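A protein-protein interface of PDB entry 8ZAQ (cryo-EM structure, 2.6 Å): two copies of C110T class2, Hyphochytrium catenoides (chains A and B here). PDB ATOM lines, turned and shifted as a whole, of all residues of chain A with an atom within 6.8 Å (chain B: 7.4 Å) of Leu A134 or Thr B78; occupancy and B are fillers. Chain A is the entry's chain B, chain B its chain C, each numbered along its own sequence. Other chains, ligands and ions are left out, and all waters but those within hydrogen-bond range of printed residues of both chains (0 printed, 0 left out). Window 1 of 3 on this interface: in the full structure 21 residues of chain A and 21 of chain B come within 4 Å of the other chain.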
ATOM      1  N   PRO A 110      30.805  -7.572  10.860  1.00  0.00           N
ATOM      2  CA  PRO A 110      31.036  -6.193  11.320  1.00  0.00           C
ATOM      3  C   PRO A 110      32.296  -6.066  12.151  1.00  0.00           C
ATOM      4  O   PRO A 110      33.177  -5.271  11.801  1.00  0.00           O
ATOM      5  CB  PRO A 110      29.780  -5.875  12.140  1.00  0.00           C
ATOM      6  CG  PRO A 110      28.745  -6.752  11.581  1.00  0.00           C
ATOM      7  CD  PRO A 110      29.448  -8.022  11.219  1.00  0.00           C
ATOM      8  N   PHE A 129      31.720  -0.037  10.462  1.00  0.00           N
ATOM      9  CA  PHE A 129      31.058  -1.029  11.301  1.00  0.00           C
ATOM     10  C   PHE A 129      29.548  -0.971  11.121  1.00  0.00           C
ATOM     11  O   PHE A 129      28.894  -1.999  10.916  1.00  0.00           O
ATOM     12  CB  PHE A 129      31.445  -0.802  12.765  1.00  0.00           C
ATOM     13  CG  PHE A 129      30.810  -1.770  13.725  1.00  0.00           C
ATOM     14  CD1 PHE A 129      29.576  -1.496  14.296  1.00  0.00           C
ATOM     15  CD2 PHE A 129      31.451  -2.946  14.066  1.00  0.00           C
ATOM     16  CE1 PHE A 129      28.993  -2.383  15.176  1.00  0.00           C
ATOM     17  CE2 PHE A 129      30.873  -3.835  14.948  1.00  0.00           C
ATOM     18  CZ  PHE A 129      29.643  -3.554  15.503  1.00  0.00           C
ATOM     19  N   PHE A 130      28.979   0.234  11.166  1.00  0.00           N
ATOM     20  CA  PHE A 130      27.532   0.362  11.050  1.00  0.00           C
ATOM     21  C   PHE A 130      27.050   0.113   9.627  1.00  0.00           C
ATOM     22  O   PHE A 130      25.936  -0.384   9.436  1.00  0.00           O
ATOM     23  CB  PHE A 130      27.088   1.733  11.551  1.00  0.00           C
ATOM     24  CG  PHE A 130      26.827   1.771  13.027  1.00  0.00           C
ATOM     25  CD1 PHE A 130      25.699   1.170  13.557  1.00  0.00           C
ATOM     26  CD2 PHE A 130      27.723   2.378  13.888  1.00  0.00           C
ATOM     27  CE1 PHE A 130      25.458   1.194  14.915  1.00  0.00           C
ATOM     28  CE2 PHE A 130      27.489   2.405  15.246  1.00  0.00           C
ATOM     29  CZ  PHE A 130      26.356   1.813  15.762  1.00  0.00           C
ATOM     30  N   ALA A 131      27.867   0.429   8.620  1.00  0.00           N
ATOM     31  CA  ALA A 131      27.500   0.097   7.248  1.00  0.00           C
ATOM     32  C   ALA A 131      27.382  -1.410   7.067  1.00  0.00           C
ATOM     33  O   ALA A 131      26.400  -1.906   6.498  1.00  0.00           O
ATOM     34  CB  ALA A 131      28.524   0.682   6.277  1.00  0.00           C
ATOM     35  N   VAL A 132      28.369  -2.158   7.563  1.00  0.00           N
ATOM     36  CA  VAL A 132      28.307  -3.616   7.489  1.00  0.00           C
ATOM     37  C   VAL A 132      27.127  -4.146   8.296  1.00  0.00           C
ATOM     38  O   VAL A 132      26.405  -5.049   7.850  1.00  0.00           O
ATOM     39  CB  VAL A 132      29.640  -4.226   7.959  1.00  0.00           C
ATOM     40  CG1 VAL A 132      29.571  -5.732   7.925  1.00  0.00           C
ATOM     41  CG2 VAL A 132      30.775  -3.740   7.084  1.00  0.00           C
ATOM     42  N   PHE A 133      26.919  -3.595   9.494  1.00  0.00           N
ATOM     43  CA  PHE A 133      25.802  -3.989  10.347  1.00  0.00           C
ATOM     44  C   PHE A 133      24.468  -3.841   9.622  1.00  0.00           C
ATOM     45  O   PHE A 133      23.646  -4.766   9.597  1.00  0.00           O
ATOM     46  CB  PHE A 133      25.831  -3.127  11.612  1.00  0.00           C
ATOM     47  CG  PHE A 133      24.996  -3.649  12.739  1.00  0.00           C
ATOM     48  CD1 PHE A 133      25.384  -4.775  13.443  1.00  0.00           C
ATOM     49  CD2 PHE A 133      23.838  -2.993  13.118  1.00  0.00           C
ATOM     50  CE1 PHE A 133      24.623  -5.244  14.491  1.00  0.00           C
ATOM     51  CE2 PHE A 133      23.074  -3.460  14.163  1.00  0.00           C
ATOM     52  CZ  PHE A 133      23.469  -4.585  14.853  1.00  0.00           C
ATOM     53  N   LEU A 134      24.247  -2.676   9.010  1.00  0.00           N
ATOM     54  CA  LEU A 134      22.975  -2.410   8.353  1.00  0.00           C
ATOM     55  C   LEU A 134      22.819  -3.234   7.084  1.00  0.00           C
ATOM     56  O   LEU A 134      21.713  -3.683   6.769  1.00  0.00           O
ATOM     57  CB  LEU A 134      22.844  -0.917   8.058  1.00  0.00           C
ATOM     58  CG  LEU A 134      22.577  -0.096   9.319  1.00  0.00           C
ATOM     59  CD1 LEU A 134      22.361   1.368   9.000  1.00  0.00           C
ATOM     60  CD2 LEU A 134      21.382  -0.669  10.056  1.00  0.00           C
ATOM     61  N   THR A 135      23.910  -3.459   6.349  1.00  0.00           N
ATOM     62  CA  THR A 135      23.835  -4.329   5.180  1.00  0.00           C
ATOM     63  C   THR A 135      23.413  -5.740   5.571  1.00  0.00           C
ATOM     64  O   THR A 135      22.538  -6.342   4.933  1.00  0.00           O
ATOM     65  CB  THR A 135      25.185  -4.357   4.466  1.00  0.00           C
ATOM     66  OG1 THR A 135      25.620  -3.017   4.208  1.00  0.00           O
ATOM     67  CG2 THR A 135      25.077  -5.111   3.160  1.00  0.00           C
ATOM     68  N   LEU A 136      24.011  -6.278   6.635  1.00  0.00           N
ATOM     69  CA  LEU A 136      23.671  -7.628   7.061  1.00  0.00           C
ATOM     70  C   LEU A 136      22.258  -7.716   7.615  1.00  0.00           C
ATOM     71  O   LEU A 136      21.572  -8.719   7.393  1.00  0.00           O
ATOM     72  CB  LEU A 136      24.678  -8.118   8.094  1.00  0.00           C
ATOM     73  CG  LEU A 136      26.067  -8.327   7.501  1.00  0.00           C
ATOM     74  CD1 LEU A 136      27.070  -8.438   8.612  1.00  0.00           C
ATOM     75  CD2 LEU A 136      26.095  -9.555   6.610  1.00  0.00           C
ATOM     76  N   TRP A 137      21.801  -6.691   8.334  1.00  0.00           N
ATOM     77  CA  TRP A 137      20.423  -6.702   8.804  1.00  0.00           C
ATOM     78  C   TRP A 137      19.419  -6.558   7.669  1.00  0.00           C
ATOM     79  O   TRP A 137      18.347  -7.167   7.730  1.00  0.00           O
ATOM     80  CB  TRP A 137      20.213  -5.608   9.848  1.00  0.00           C
ATOM     81  CG  TRP A 137      20.535  -6.092  11.219  1.00  0.00           C
ATOM     82  CD1 TRP A 137      21.540  -5.659  12.025  1.00  0.00           C
ATOM     83  CD2 TRP A 137      19.867  -7.137  11.936  1.00  0.00           C
ATOM     84  NE1 TRP A 137      21.531  -6.354  13.206  1.00  0.00           N
ATOM     85  CE2 TRP A 137      20.513  -7.268  13.177  1.00  0.00           C
ATOM     86  CE3 TRP A 137      18.779  -7.966  11.652  1.00  0.00           C
ATOM     87  CZ2 TRP A 137      20.110  -8.195  14.133  1.00  0.00           C
ATOM     88  CZ3 TRP A 137      18.381  -8.883  12.601  1.00  0.00           C
ATOM     89  CH2 TRP A 137      19.044  -8.991  13.826  1.00  0.00           C
ATOM     90  N   CYS A 138      19.748  -5.789   6.632  1.00  0.00           N
ATOM     91  CA  CYS A 138      18.918  -5.765   5.436  1.00  0.00           C
ATOM     92  C   CYS A 138      18.864  -7.129   4.767  1.00  0.00           C
ATOM     93  O   CYS A 138      17.806  -7.531   4.279  1.00  0.00           O
ATOM     94  CB  CYS A 138      19.436  -4.717   4.451  1.00  0.00           C
ATOM     95  SG  CYS A 138      19.230  -3.010   4.984  1.00  0.00           S
ATOM     96  N   GLY A 139      19.988  -7.848   4.730  1.00  0.00           N
ATOM     97  CA  GLY A 139      19.967  -9.212   4.225  1.00  0.00           C
ATOM     98  C   GLY A 139      19.120 -10.161   5.047  1.00  0.00           C
ATOM     99  O   GLY A 139      18.401 -10.997   4.488  1.00  0.00           O
ATOM    100  N   TYR A 153      14.240  -5.006   0.596  1.00  0.00           N
ATOM    101  CA  TYR A 153      15.258  -5.110   1.633  1.00  0.00           C
ATOM    102  C   TYR A 153      16.628  -5.379   1.038  1.00  0.00           C
ATOM    103  O   TYR A 153      17.595  -4.689   1.381  1.00  0.00           O
ATOM    104  CB  TYR A 153      14.897  -6.220   2.617  1.00  0.00           C
ATOM    105  CG  TYR A 153      13.841  -5.840   3.621  1.00  0.00           C
ATOM    106  CD1 TYR A 153      14.061  -4.821   4.536  1.00  0.00           C
ATOM    107  CD2 TYR A 153      12.622  -6.496   3.651  1.00  0.00           C
ATOM    108  CE1 TYR A 153      13.097  -4.475   5.458  1.00  0.00           C
ATOM    109  CE2 TYR A 153      11.653  -6.153   4.565  1.00  0.00           C
ATOM    110  CZ  TYR A 153      11.894  -5.143   5.466  1.00  0.00           C
ATOM    111  OH  TYR A 153      10.926  -4.803   6.378  1.00  0.00           O
ATOM    112  N   LEU A 156      17.780  -2.268  -0.310  1.00  0.00           N
ATOM    113  CA  LEU A 156      18.261  -1.456   0.799  1.00  0.00           C
ATOM    114  C   LEU A 156      19.670  -1.870   1.195  1.00  0.00           C
ATOM    115  O   LEU A 156      20.552  -1.017   1.348  1.00  0.00           O
ATOM    116  CB  LEU A 156      17.304  -1.570   1.985  1.00  0.00           C
ATOM    117  CG  LEU A 156      17.422  -0.520   3.091  1.00  0.00           C
ATOM    118  CD1 LEU A 156      17.326   0.884   2.520  1.00  0.00           C
ATOM    119  CD2 LEU A 156      16.361  -0.746   4.153  1.00  0.00           C
ATOM    120  N   GLY A 157      19.913  -3.179   1.311  1.00  0.00           N
ATOM    121  CA  GLY A 157      21.261  -3.648   1.563  1.00  0.00           C
ATOM    122  C   GLY A 157      22.243  -3.264   0.485  1.00  0.00           C
ATOM    123  O   GLY A 157      23.361  -2.846   0.800  1.00  0.00           O
ATOM    124  N   TRP A 160      23.563   0.083   0.948  1.00  0.00           N
ATOM    125  CA  TRP A 160      24.532   0.255   2.017  1.00  0.00           C
ATOM    126  C   TRP A 160      25.867  -0.409   1.730  1.00  0.00           C
ATOM    127  O   TRP A 160      26.894   0.063   2.220  1.00  0.00           O
ATOM    128  CB  TRP A 160      23.975  -0.300   3.334  1.00  0.00           C
ATOM    129  CG  TRP A 160      23.284   0.728   4.168  1.00  0.00           C
ATOM    130  CD1 TRP A 160      21.940   0.882   4.330  1.00  0.00           C
ATOM    131  CD2 TRP A 160      23.903   1.745   4.963  1.00  0.00           C
ATOM    132  NE1 TRP A 160      21.681   1.935   5.171  1.00  0.00           N
ATOM    133  CE2 TRP A 160      22.871   2.482   5.574  1.00  0.00           C
ATOM    134  CE3 TRP A 160      25.231   2.105   5.215  1.00  0.00           C
ATOM    135  CZ2 TRP A 160      23.123   3.557   6.421  1.00  0.00           C
ATOM    136  CZ3 TRP A 160      25.478   3.171   6.057  1.00  0.00           C
ATOM    137  CH2 TRP A 160      24.431   3.884   6.650  1.00  0.00           C
ATOM    138  N   CYS B  31       9.876  10.068   5.913  1.00  0.00           N
ATOM    139  CA  CYS B  31      10.749  10.158   7.077  1.00  0.00           C
ATOM    140  C   CYS B  31      12.093   9.497   6.809  1.00  0.00           C
ATOM    141  O   CYS B  31      13.135  10.023   7.204  1.00  0.00           O
ATOM    142  CB  CYS B  31      10.073   9.528   8.295  1.00  0.00           C
ATOM    143  SG  CYS B  31       8.760  10.527   9.017  1.00  0.00           S
ATOM    144  N   CYS B  32      12.090   8.340   6.146  1.00  0.00           N
ATOM    145  CA  CYS B  32      13.334   7.673   5.790  1.00  0.00           C
ATOM    146  C   CYS B  32      14.211   8.580   4.945  1.00  0.00           C
ATOM    147  O   CYS B  32      15.397   8.768   5.233  1.00  0.00           O
ATOM    148  CB  CYS B  32      13.034   6.374   5.041  1.00  0.00           C
ATOM    149  SG  CYS B  32      14.365   5.833   3.948  1.00  0.00           S
ATOM    150  N   VAL B  33      13.628   9.169   3.900  1.00  0.00           N
ATOM    151  CA  VAL B  33      14.400  10.038   3.020  1.00  0.00           C
ATOM    152  C   VAL B  33      14.968  11.216   3.799  1.00  0.00           C
ATOM    153  O   VAL B  33      16.162  11.521   3.701  1.00  0.00           O
ATOM    154  CB  VAL B  33      13.541  10.507   1.832  1.00  0.00           C
ATOM    155  CG1 VAL B  33      14.284  11.552   1.019  1.00  0.00           C
ATOM    156  CG2 VAL B  33      13.166   9.328   0.955  1.00  0.00           C
ATOM    157  N   VAL B  35      15.456  11.716   7.145  1.00  0.00           N
ATOM    158  CA  VAL B  35      16.413  11.387   8.198  1.00  0.00           C
ATOM    159  C   VAL B  35      17.718  10.870   7.603  1.00  0.00           C
ATOM    160  O   VAL B  35      18.808  11.222   8.071  1.00  0.00           O
ATOM    161  CB  VAL B  35      15.798  10.382   9.191  1.00  0.00           C
ATOM    162  CG1 VAL B  35      16.754  10.114  10.331  1.00  0.00           C
ATOM    163  CG2 VAL B  35      14.491  10.914   9.747  1.00  0.00           C
ATOM    164  N   ALA B  36      17.636  10.030   6.565  1.00  0.00           N
ATOM    165  CA  ALA B  36      18.847   9.539   5.920  1.00  0.00           C
ATOM    166  C   ALA B  36      19.619  10.671   5.258  1.00  0.00           C
ATOM    167  O   ALA B  36      20.851  10.716   5.341  1.00  0.00           O
ATOM    168  CB  ALA B  36      18.495   8.455   4.904  1.00  0.00           C
ATOM    169  N   ILE B  71      25.586   8.817  11.924  1.00  0.00           N
ATOM    170  CA  ILE B  71      25.394   7.369  11.930  1.00  0.00           C
ATOM    171  C   ILE B  71      24.019   7.014  12.479  1.00  0.00           C
ATOM    172  O   ILE B  71      23.314   6.164  11.927  1.00  0.00           O
ATOM    173  CB  ILE B  71      26.521   6.689  12.729  1.00  0.00           C
ATOM    174  CG1 ILE B  71      27.746   6.467  11.841  1.00  0.00           C
ATOM    175  CG2 ILE B  71      26.046   5.376  13.328  1.00  0.00           C
ATOM    176  CD1 ILE B  71      29.021   6.255  12.613  1.00  0.00           C
ATOM    177  N   ILE B  72      23.620   7.659  13.575  1.00  0.00           N
ATOM    178  CA  ILE B  72      22.309   7.417  14.167  1.00  0.00           C
ATOM    179  C   ILE B  72      21.206   7.844  13.214  1.00  0.00           C
ATOM    180  O   ILE B  72      20.196   7.149  13.066  1.00  0.00           O
ATOM    181  CB  ILE B  72      22.198   8.131  15.527  1.00  0.00           C
ATOM    182  CG1 ILE B  72      23.070   7.433  16.569  1.00  0.00           C
ATOM    183  CG2 ILE B  72      20.753   8.190  15.998  1.00  0.00           C
ATOM    184  CD1 ILE B  72      23.604   8.361  17.622  1.00  0.00           C
ATOM    185  N   CYS B  73      21.369   8.994  12.558  1.00  0.00           N
ATOM    186  CA  CYS B  73      20.357   9.425  11.601  1.00  0.00           C
ATOM    187  C   CYS B  73      20.248   8.468  10.420  1.00  0.00           C
ATOM    188  O   CYS B  73      19.139   8.164   9.974  1.00  0.00           O
ATOM    189  CB  CYS B  73      20.654  10.844  11.125  1.00  0.00           C
ATOM    190  SG  CYS B  73      19.846  12.122  12.103  1.00  0.00           S
ATOM    191  N   LEU B  74      21.374   7.974   9.905  1.00  0.00           N
ATOM    192  CA  LEU B  74      21.329   7.008   8.812  1.00  0.00           C
ATOM    193  C   LEU B  74      20.724   5.678   9.243  1.00  0.00           C
ATOM    194  O   LEU B  74      19.984   5.063   8.471  1.00  0.00           O
ATOM    195  CB  LEU B  74      22.731   6.796   8.243  1.00  0.00           C
ATOM    196  CG  LEU B  74      23.135   7.821   7.184  1.00  0.00           C
ATOM    197  CD1 LEU B  74      24.638   8.005   7.160  1.00  0.00           C
ATOM    198  CD2 LEU B  74      22.618   7.411   5.818  1.00  0.00           C
ATOM    199  N   LEU B  75      21.025   5.221  10.459  1.00  0.00           N
ATOM    200  CA  LEU B  75      20.408   4.003  10.973  1.00  0.00           C
ATOM    201  C   LEU B  75      18.903   4.173  11.146  1.00  0.00           C
ATOM    202  O   LEU B  75      18.127   3.270  10.816  1.00  0.00           O
ATOM    203  CB  LEU B  75      21.073   3.606  12.290  1.00  0.00           C
ATOM    204  CG  LEU B  75      20.307   2.720  13.273  1.00  0.00           C
ATOM    205  CD1 LEU B  75      20.455   1.257  12.919  1.00  0.00           C
ATOM    206  CD2 LEU B  75      20.817   2.971  14.679  1.00  0.00           C
ATOM    207  N   CYS B  76      18.471   5.329  11.653  1.00  0.00           N
ATOM    208  CA  CYS B  76      17.044   5.598  11.787  1.00  0.00           C
ATOM    209  C   CYS B  76      16.369   5.682  10.423  1.00  0.00           C
ATOM    210  O   CYS B  76      15.238   5.217  10.259  1.00  0.00           O
ATOM    211  CB  CYS B  76      16.830   6.885  12.585  1.00  0.00           C
ATOM    212  SG  CYS B  76      15.113   7.413  12.743  1.00  0.00           S
ATOM    213  N   GLY B  77      17.046   6.265   9.432  1.00  0.00           N
ATOM    214  CA  GLY B  77      16.489   6.306   8.089  1.00  0.00           C
ATOM    215  C   GLY B  77      16.383   4.933   7.452  1.00  0.00           C
ATOM    216  O   GLY B  77      15.416   4.638   6.746  1.00  0.00           O
ATOM    217  N   THR B  78      17.382   4.077   7.678  1.00  0.00           N
ATOM    218  CA  THR B  78      17.291   2.696   7.219  1.00  0.00           C
ATOM    219  C   THR B  78      16.143   1.957   7.896  1.00  0.00           C
ATOM    220  O   THR B  78      15.404   1.212   7.237  1.00  0.00           O
ATOM    221  CB  THR B  78      18.612   1.971   7.478  1.00  0.00           C
ATOM    222  OG1 THR B  78      19.702   2.864   7.223  1.00  0.00           O
ATOM    223  CG2 THR B  78      18.743   0.751   6.584  1.00  0.00           C
ATOM    224  N   MET B  79      15.976   2.155   9.203  1.00  0.00           N
ATOM    225  CA  MET B  79      14.859   1.528   9.899  1.00  0.00           C
ATOM    226  C   MET B  79      13.527   2.069   9.399  1.00  0.00           C
ATOM    227  O   MET B  79      12.539   1.335   9.355  1.00  0.00           O
ATOM    228  CB  MET B  79      14.992   1.721  11.407  1.00  0.00           C
ATOM    229  CG  MET B  79      16.205   1.040  12.009  1.00  0.00           C
ATOM    230  SD  MET B  79      16.162   1.051  13.805  1.00  0.00           S
ATOM    231  CE  MET B  79      15.753   2.766  14.102  1.00  0.00           C
ATOM    232  N   TYR B  80      13.477   3.340   9.003  1.00  0.00           N
ATOM    233  CA  TYR B  80      12.247   3.878   8.434  1.00  0.00           C
ATOM    234  C   TYR B  80      11.985   3.365   7.025  1.00  0.00           C
ATOM    235  O   TYR B  80      10.822   3.222   6.643  1.00  0.00           O
ATOM    236  CB  TYR B  80      12.270   5.404   8.445  1.00  0.00           C
ATOM    237  CG  TYR B  80      11.569   5.976   9.649  1.00  0.00           C
ATOM    238  CD1 TYR B  80      12.283   6.358  10.774  1.00  0.00           C
ATOM    239  CD2 TYR B  80      10.189   6.091   9.679  1.00  0.00           C
ATOM    240  CE1 TYR B  80      11.644   6.862  11.883  1.00  0.00           C
ATOM    241  CE2 TYR B  80       9.541   6.593  10.785  1.00  0.00           C
ATOM    242  CZ  TYR B  80      10.274   6.977  11.883  1.00  0.00           C
ATOM    243  OH  TYR B  80       9.637   7.477  12.992  1.00  0.00           O
ATOM    244  N   ALA B  81      13.031   3.082   6.249  1.00  0.00           N
ATOM    245  CA  ALA B  81      12.836   2.381   4.982  1.00  0.00           C
ATOM    246  C   ALA B  81      12.255   0.992   5.213  1.00  0.00           C
ATOM    247  O   ALA B  81      11.332   0.569   4.509  1.00  0.00           O
ATOM    248  CB  ALA B  81      14.156   2.289   4.220  1.00  0.00           C
ATOM    249  N   ALA B  82      12.777   0.278   6.211  1.00  0.00           N
ATOM    250  CA  ALA B  82      12.206  -1.017   6.573  1.00  0.00           C
ATOM    251  C   ALA B  82      10.764  -0.886   7.055  1.00  0.00           C
ATOM    252  O   ALA B  82       9.922  -1.732   6.735  1.00  0.00           O
ATOM    253  CB  ALA B  82      13.068  -1.686   7.642  1.00  0.00           C
ATOM    254  N   LYS B  83      10.467   0.159   7.829  1.00  0.00           N
ATOM    255  CA  LYS B  83       9.104   0.414   8.281  1.00  0.00           C
ATOM    256  C   LYS B  83       8.169   0.694   7.117  1.00  0.00           C
ATOM    257  O   LYS B  83       7.019   0.250   7.126  1.00  0.00           O
ATOM    258  CB  LYS B  83       9.085   1.594   9.249  1.00  0.00           C
ATOM    259  CG  LYS B  83       9.675   1.318  10.611  1.00  0.00           C
ATOM    260  CD  LYS B  83       9.863   2.619  11.368  1.00  0.00           C
ATOM    261  CE  LYS B  83      10.629   2.408  12.654  1.00  0.00           C
ATOM    262  NZ  LYS B  83       9.726   2.481  13.833  1.00  0.00           N
ATOM    263  N   SER B  84       8.635   1.454   6.126  1.00  0.00           N
ATOM    264  CA  SER B  84       7.842   1.695   4.928  1.00  0.00           C
ATOM    265  C   SER B  84       7.608   0.401   4.159  1.00  0.00           C
ATOM    266  O   SER B  84       6.516   0.180   3.627  1.00  0.00           O
ATOM    267  CB  SER B  84       8.535   2.734   4.048  1.00  0.00           C
ATOM    268  OG  SER B  84       8.055   2.688   2.719  1.00  0.00           O
ATOM    269  N   PHE B  85       8.624  -0.464   4.090  1.00  0.00           N
ATOM    270  CA  PHE B  85       8.437  -1.771   3.466  1.00  0.00           C
ATOM    271  C   PHE B  85       7.370  -2.576   4.195  1.00  0.00           C
ATOM    272  O   PHE B  85       6.519  -3.211   3.562  1.00  0.00           O
ATOM    273  CB  PHE B  85       9.754  -2.552   3.444  1.00  0.00           C
ATOM    274  CG  PHE B  85      10.860  -1.880   2.678  1.00  0.00           C
ATOM    275  CD1 PHE B  85      10.587  -0.909   1.729  1.00  0.00           C
ATOM    276  CD2 PHE B  85      12.181  -2.228   2.910  1.00  0.00           C
ATOM    277  CE1 PHE B  85      11.609  -0.296   1.033  1.00  0.00           C
ATOM    278  CE2 PHE B  85      13.204  -1.619   2.219  1.00  0.00           C
ATOM    279  CZ  PHE B  85      12.919  -0.652   1.279  1.00  0.00           C
ATOM    280  N   LEU B  97       9.692  -3.562  11.798  1.00  0.00           N
ATOM    281  CA  LEU B  97      10.260  -2.590  12.717  1.00  0.00           C
ATOM    282  C   LEU B  97       9.197  -1.661  13.280  1.00  0.00           C
ATOM    283  O   LEU B  97       9.521  -0.730  14.023  1.00  0.00           O
ATOM    284  CB  LEU B  97      11.366  -1.793  12.027  1.00  0.00           C
ATOM    285  CG  LEU B  97      12.614  -2.608  11.679  1.00  0.00           C
ATOM    286  CD1 LEU B  97      13.741  -1.709  11.222  1.00  0.00           C
ATOM    287  CD2 LEU B  97      13.051  -3.462  12.857  1.00  0.00           C
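O of Leu A134 sits at hydrogen-bond distance from SG of Cys A138 (3.1 Å).
OG1 of Thr B78 sits at hydrogen-bond distance from O of Leu B74 (2.5 Å).
CG2 of Ile B71 touches CD2 of Phe A130, at 3.5 Å.
Leu A134 touches Leu B75.
CD1 of Leu A134 touches OG1 of Thr B78 (3.5 Å).
Tyr A153 touches Phe B85 (CE1 to CD2, 3.5 Å).
Leu A156 touches Thr B78 (CD2 to CG2, 3.7 Å).
CD2 of Leu A156 touches CB of Ala B81, 3.8 Å away.
Leu A156 touches Phe B85.
Trp A160 touches Leu B74 (CH2 to CB, 3.7 Å).
Hydrophobic or aromatic side chains of chain B that line the printed part of chain A: Ile B71, Leu B74, Leu B75, Ala B81, Ala B82 and Phe B85.
Printed residues of chain A that touch a printed residue of chain B: Phe A130, Leu A134, Tyr A153, Leu A156 and Trp A160.
Among the printed residues, 10 pairs touch across the chains.
Among the printed residues, no Asp or Glu carboxylate lies within 4 Å of a Lys or Arg side-chain nitrogen of the other chain.
OH of Tyr A153 sits at hydrogen-bond distance from O of Ala B82.
The side-chain hydroxyl (OG1) of Thr B78 is in hydrogen-bond range of the indole nitrogen (NE1) of Trp A160.
Leu A134 touches two residues of chain B.
Cys B32 touches none of the printed residues of chain A.
Gly B77 touches none of the printed residues of chain A.
Of chain A, only Leu A134, Leu A156 and Trp A160 come within 4 Å of Thr B78.
Of the printed residues of chain A, Ala B81 touches Leu A156 (3.8 Å).
Printed residues of chain A within 4 Å of Ala B82: Tyr A153.
The nearest printed residue of chain B that does not touch Phe A130 is Leu B75 (5.0 Å).
No position is printed for both chains.
Of the 10 pairs that touch across the chains among the printed residues, none has its exchanged pair printed and touching as well.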
